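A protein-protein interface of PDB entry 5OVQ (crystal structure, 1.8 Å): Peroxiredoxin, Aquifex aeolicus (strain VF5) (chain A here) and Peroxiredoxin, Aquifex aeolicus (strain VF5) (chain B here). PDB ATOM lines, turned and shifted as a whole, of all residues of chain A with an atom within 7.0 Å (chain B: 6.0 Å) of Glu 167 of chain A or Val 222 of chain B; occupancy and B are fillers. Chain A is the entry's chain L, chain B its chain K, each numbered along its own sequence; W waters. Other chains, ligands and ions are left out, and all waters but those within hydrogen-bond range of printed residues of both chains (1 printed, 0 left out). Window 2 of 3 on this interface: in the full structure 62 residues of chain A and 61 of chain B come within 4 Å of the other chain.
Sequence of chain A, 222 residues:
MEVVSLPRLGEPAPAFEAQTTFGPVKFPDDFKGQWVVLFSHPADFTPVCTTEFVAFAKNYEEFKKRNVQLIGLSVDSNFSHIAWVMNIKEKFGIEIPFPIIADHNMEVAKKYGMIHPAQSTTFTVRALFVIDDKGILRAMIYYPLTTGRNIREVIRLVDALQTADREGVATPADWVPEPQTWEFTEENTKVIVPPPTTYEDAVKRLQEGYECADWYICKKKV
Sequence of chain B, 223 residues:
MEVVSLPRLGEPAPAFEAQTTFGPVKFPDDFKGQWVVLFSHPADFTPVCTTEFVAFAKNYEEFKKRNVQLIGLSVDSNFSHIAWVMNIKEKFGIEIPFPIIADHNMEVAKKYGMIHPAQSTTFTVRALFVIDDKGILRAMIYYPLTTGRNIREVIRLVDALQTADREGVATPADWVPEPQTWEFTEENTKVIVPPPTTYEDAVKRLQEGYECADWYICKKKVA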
ATOM      1  N   GLN A 162     -26.383 -10.122  11.496  1.00  0.00           N
ATOM      2  CA  GLN A 162     -25.062 -10.722  11.374  1.00  0.00           C
ATOM      3  C   GLN A 162     -25.056 -12.140  11.941  1.00  0.00           C
ATOM      4  O   GLN A 162     -24.370 -13.021  11.415  1.00  0.00           O
ATOM      5  CB  GLN A 162     -24.030  -9.846  12.087  1.00  0.00           C
ATOM      6  CG  GLN A 162     -23.900  -8.497  11.417  1.00  0.00           C
ATOM      7  CD  GLN A 162     -22.857  -7.601  12.072  1.00  0.00           C
ATOM      8  OE1 GLN A 162     -22.468  -7.820  13.211  1.00  0.00           O
ATOM      9  NE2 GLN A 162     -22.436  -6.561  11.360  1.00  0.00           N
ATOM     10  N   THR A 163     -25.800 -12.370  13.026  1.00  0.00           N
ATOM     11  CA  THR A 163     -25.892 -13.722  13.569  1.00  0.00           C
ATOM     12  C   THR A 163     -26.609 -14.651  12.600  1.00  0.00           C
ATOM     13  O   THR A 163     -26.155 -15.775  12.360  1.00  0.00           O
ATOM     14  CB  THR A 163     -26.600 -13.702  14.926  1.00  0.00           C
ATOM     15  OG1 THR A 163     -25.792 -13.001  15.879  1.00  0.00           O
ATOM     16  CG2 THR A 163     -26.856 -15.119  15.430  1.00  0.00           C
ATOM     17  N   ALA A 164     -27.709 -14.179  12.008  1.00  0.00           N
ATOM     18  CA  ALA A 164     -28.433 -14.973  11.021  1.00  0.00           C
ATOM     19  C   ALA A 164     -27.520 -15.402   9.879  1.00  0.00           C
ATOM     20  O   ALA A 164     -27.491 -16.578   9.500  1.00  0.00           O
ATOM     21  CB  ALA A 164     -29.626 -14.170  10.494  1.00  0.00           C
ATOM     22  N   ASP A 165     -26.755 -14.460   9.326  1.00  0.00           N
ATOM     23  CA  ASP A 165     -25.848 -14.784   8.228  1.00  0.00           C
ATOM     24  C   ASP A 165     -24.744 -15.735   8.675  1.00  0.00           C
ATOM     25  O   ASP A 165     -24.434 -16.710   7.984  1.00  0.00           O
ATOM     26  CB  ASP A 165     -25.224 -13.511   7.662  1.00  0.00           C
ATOM     27  CG  ASP A 165     -26.215 -12.647   6.912  1.00  0.00           C
ATOM     28  OD1 ASP A 165     -27.399 -13.022   6.803  1.00  0.00           O
ATOM     29  OD2 ASP A 165     -25.793 -11.587   6.420  1.00  0.00           O
ATOM     30  N   ARG A 166     -24.129 -15.458   9.829  1.00  0.00           N
ATOM     31  CA  ARG A 166     -22.960 -16.223  10.250  1.00  0.00           C
ATOM     32  C   ARG A 166     -23.316 -17.659  10.609  1.00  0.00           C
ATOM     33  O   ARG A 166     -22.581 -18.589  10.261  1.00  0.00           O
ATOM     34  CB  ARG A 166     -22.294 -15.549  11.447  1.00  0.00           C
ATOM     35  CG  ARG A 166     -21.032 -16.256  11.916  1.00  0.00           C
ATOM     36  CD  ARG A 166     -20.478 -15.644  13.193  1.00  0.00           C
ATOM     37  NE  ARG A 166     -21.397 -15.764  14.324  1.00  0.00           N
ATOM     38  CZ  ARG A 166     -22.093 -14.750  14.828  1.00  0.00           C
ATOM     39  NH1 ARG A 166     -21.978 -13.534  14.303  1.00  0.00           N
ATOM     40  NH2 ARG A 166     -22.904 -14.950  15.858  1.00  0.00           N
ATOM     41  N   GLU A 167     -24.419 -17.857  11.325  1.00  0.00           N
ATOM     42  CA  GLU A 167     -24.769 -19.163  11.868  1.00  0.00           C
ATOM     43  C   GLU A 167     -25.844 -19.878  11.073  1.00  0.00           C
ATOM     44  O   GLU A 167     -26.138 -21.040  11.371  1.00  0.00           O
ATOM     45  CB  GLU A 167     -25.209 -19.030  13.330  1.00  0.00           C
ATOM     46  CG  GLU A 167     -24.168 -18.364  14.226  1.00  0.00           C
ATOM     47  CD  GLU A 167     -22.962 -19.259  14.473  1.00  0.00           C
ATOM     48  OE1 GLU A 167     -23.097 -20.494  14.324  1.00  0.00           O
ATOM     49  OE2 GLU A 167     -21.886 -18.734  14.824  1.00  0.00           O
ATOM     50  N   GLY A 168     -26.441 -19.220  10.085  1.00  0.00           N
ATOM     51  CA  GLY A 168     -27.531 -19.815   9.330  1.00  0.00           C
ATOM     52  C   GLY A 168     -28.769 -20.064  10.159  1.00  0.00           C
ATOM     53  O   GLY A 168     -29.354 -21.155  10.092  1.00  0.00           O
ATOM     54  N   VAL A 169     -29.162 -19.094  10.974  1.00  0.00           N
ATOM     55  CA  VAL A 169     -30.274 -19.246  11.894  1.00  0.00           C
ATOM     56  C   VAL A 169     -31.188 -18.042  11.746  1.00  0.00           C
ATOM     57  O   VAL A 169     -30.874 -17.076  11.056  1.00  0.00           O
ATOM     58  CB  VAL A 169     -29.802 -19.371  13.352  1.00  0.00           C
ATOM     59  CG1 VAL A 169     -28.907 -20.586  13.523  1.00  0.00           C
ATOM     60  CG2 VAL A 169     -29.061 -18.084  13.764  1.00  0.00           C
ATOM     61  N   ALA A 170     -32.336 -18.116  12.406  1.00  0.00           N
ATOM     62  CA  ALA A 170     -33.203 -16.964  12.579  1.00  0.00           C
ATOM     63  C   ALA A 170     -33.190 -16.539  14.039  1.00  0.00           C
ATOM     64  O   ALA A 170     -32.786 -17.297  14.925  1.00  0.00           O
ATOM     65  CB  ALA A 170     -34.631 -17.276  12.104  1.00  0.00           C
ATOM     66  N   TRP A 175     -34.693 -11.077  20.676  1.00  0.00           N
ATOM     67  CA  TRP A 175     -33.421 -11.788  20.753  1.00  0.00           C
ATOM     68  C   TRP A 175     -32.249 -10.851  21.008  1.00  0.00           C
ATOM     69  O   TRP A 175     -32.157  -9.783  20.406  1.00  0.00           O
ATOM     70  CB  TRP A 175     -33.157 -12.536  19.455  1.00  0.00           C
ATOM     71  CG  TRP A 175     -31.855 -13.242  19.452  1.00  0.00           C
ATOM     72  CD1 TRP A 175     -31.599 -14.495  19.937  1.00  0.00           C
ATOM     73  CD2 TRP A 175     -30.615 -12.741  18.957  1.00  0.00           C
ATOM     74  NE1 TRP A 175     -30.277 -14.809  19.756  1.00  0.00           N
ATOM     75  CE2 TRP A 175     -29.650 -13.744  19.156  1.00  0.00           C
ATOM     76  CE3 TRP A 175     -30.225 -11.536  18.361  1.00  0.00           C
ATOM     77  CZ2 TRP A 175     -28.314 -13.580  18.783  1.00  0.00           C
ATOM     78  CZ3 TRP A 175     -28.898 -11.373  17.988  1.00  0.00           C
ATOM     79  CH2 TRP A 175     -27.957 -12.392  18.208  1.00  0.00           C
ATOM     80  N   PRO A 177     -27.687 -11.315  21.629  1.00  0.00           N
ATOM     81  CA  PRO A 177     -26.606 -12.318  21.572  1.00  0.00           C
ATOM     82  C   PRO A 177     -26.116 -12.779  22.935  1.00  0.00           C
ATOM     83  O   PRO A 177     -25.630 -13.911  23.056  1.00  0.00           O
ATOM     84  CB  PRO A 177     -25.495 -11.600  20.793  1.00  0.00           C
ATOM     85  CG  PRO A 177     -25.789 -10.155  20.946  1.00  0.00           C
ATOM     86  CD  PRO A 177     -27.277 -10.029  21.031  1.00  0.00           C
ATOM     87  N   THR B 189     -31.321 -15.394  24.283  1.00  0.00           N
ATOM     88  CA  THR B 189     -30.169 -15.631  23.426  1.00  0.00           C
ATOM     89  C   THR B 189     -30.321 -16.854  22.540  1.00  0.00           C
ATOM     90  O   THR B 189     -29.515 -17.040  21.624  1.00  0.00           O
ATOM     91  CB  THR B 189     -28.902 -15.790  24.269  1.00  0.00           C
ATOM     92  OG1 THR B 189     -28.960 -17.020  25.011  1.00  0.00           O
ATOM     93  CG2 THR B 189     -28.777 -14.622  25.225  1.00  0.00           C
ATOM     94  N   VAL B 191     -31.240 -19.017  19.545  1.00  0.00           N
ATOM     95  CA  VAL B 191     -31.591 -18.761  18.170  1.00  0.00           C
ATOM     96  C   VAL B 191     -32.527 -19.857  17.683  1.00  0.00           C
ATOM     97  O   VAL B 191     -32.757 -20.864  18.357  1.00  0.00           O
ATOM     98  CB  VAL B 191     -30.353 -18.651  17.263  1.00  0.00           C
ATOM     99  CG1 VAL B 191     -29.522 -17.445  17.659  1.00  0.00           C
ATOM    100  CG2 VAL B 191     -29.528 -19.907  17.358  1.00  0.00           C
ATOM    101  N   LYS B 220     -31.746 -23.363  19.732  1.00  0.00           N
ATOM    102  CA  LYS B 220     -30.441 -23.777  20.222  1.00  0.00           C
ATOM    103  C   LYS B 220     -29.686 -22.528  20.642  1.00  0.00           C
ATOM    104  O   LYS B 220     -30.155 -21.403  20.451  1.00  0.00           O
ATOM    105  CB  LYS B 220     -29.661 -24.550  19.155  1.00  0.00           C
ATOM    106  CG  LYS B 220     -29.369 -23.756  17.890  1.00  0.00           C
ATOM    107  CD  LYS B 220     -28.458 -24.538  16.964  1.00  0.00           C
ATOM    108  CE  LYS B 220     -27.953 -23.672  15.821  1.00  0.00           C
ATOM    109  NZ  LYS B 220     -27.032 -24.408  14.909  1.00  0.00           N
ATOM    110  N   LYS B 221     -28.502 -22.725  21.203  1.00  0.00           N
ATOM    111  CA  LYS B 221     -27.615 -21.603  21.459  1.00  0.00           C
ATOM    112  C   LYS B 221     -26.425 -21.655  20.509  1.00  0.00           C
ATOM    113  O   LYS B 221     -26.017 -22.725  20.056  1.00  0.00           O
ATOM    114  CB  LYS B 221     -27.139 -21.609  22.909  1.00  0.00           C
ATOM    115  CG  LYS B 221     -28.246 -21.286  23.890  1.00  0.00           C
ATOM    116  CD  LYS B 221     -27.729 -21.228  25.304  1.00  0.00           C
ATOM    117  CE  LYS B 221     -28.863 -20.970  26.269  1.00  0.00           C
ATOM    118  NZ  LYS B 221     -28.345 -20.961  27.655  1.00  0.00           N
ATOM    119  N   VAL B 222     -25.874 -20.485  20.194  1.00  0.00           N
ATOM    120  CA  VAL B 222     -24.682 -20.442  19.352  1.00  0.00           C
ATOM    121  C   VAL B 222     -23.513 -19.793  20.085  1.00  0.00           C
ATOM    122  O   VAL B 222     -23.706 -18.889  20.898  1.00  0.00           O
ATOM    123  CB  VAL B 222     -24.970 -19.733  18.024  1.00  0.00           C
ATOM    124  CG1 VAL B 222     -25.876 -20.606  17.162  1.00  0.00           C
ATOM    125  CG2 VAL B 222     -25.618 -18.387  18.277  1.00  0.00           C
ATOM    126  N   ALA B 223     -22.301 -20.254  19.784  1.00  0.00           N
ATOM    127  CA  ALA B 223     -21.086 -19.659  20.334  1.00  0.00           C
ATOM    128  C   ALA B 223     -20.714 -18.391  19.567  1.00  0.00           C
ATOM    129  O   ALA B 223     -20.726 -17.282  20.110  1.00  0.00           O
ATOM    130  CB  ALA B 223     -19.928 -20.658  20.292  1.00  0.00           C
HETATM  131  O   HOH W   1     -24.994 -23.002  13.303  1.00  0.00           O
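The backbone carbonyl oxygen of Thr 189 of chain B lies within hydrogen-bond range of the indole nitrogen of Trp 175 of chain A, 3.0 Å away.
The backbone NH (N) of Val 191 of chain B is in hydrogen-bond range of the backbone carbonyl oxygen (O) of Lys 220 of chain B.
O of Ala 164 of chain A lies within hydrogen-bond range of N of Val 169 of chain A, at 3.4 Å.
The guanidinium group (NE) of Arg 166 of chain A lies within salt-bridge range of the side-chain carboxylate (OE2) of Glu 167 of chain A, 3.1 Å away.
CG1 of Val 222 of chain B touches OE1 of Glu 167 of chain A, 3.97 Å away.
Val 169 of chain A touches Val 191 of chain B.
CG1 of Val 169 of chain A touches CE of Lys 220 of chain B, at 3.96 Å.
Ala 170 of chain A touches Val 191 of chain B (O to CB, 3.6 Å).
Trp 175 of chain A touches Val 191 of chain B (NE1 to CG1, 3.5 Å).
Pro 177 of chain A touches Thr 189 of chain B.
Gly 168 of chain A touches none of the printed residues of chain B.
Printed residues of chain B within 4 Å of Ala 170 of chain A: Val 191.
Of the printed residues of chain B, Pro 177 of chain A touches Thr 189.
Printed residues of chain A within 4 Å of Thr 189 of chain B: Trp 175 and Pro 177.
Val 222 of chain B touches just one residue of chain A: Glu 167.
The nearest residue of chain B that does not touch Glu 167 of chain A is Ala 223 of chain B (4.9 Å).
Of the 6 printed residues of chain B, 4 touch a printed residue of chain A.
Hydrophobic or aromatic side chains of chain B that line the printed part of chain A: Val 191 and Val 222.
Among the printed residues, no Asp or Glu carboxylate lies within 4 Å of a Lys or Arg side-chain nitrogen of the other chain.
Water W1 lies within hydrogen-bond range of NZ of Lys 220 of chain B and O of Glu 167 of chain A.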
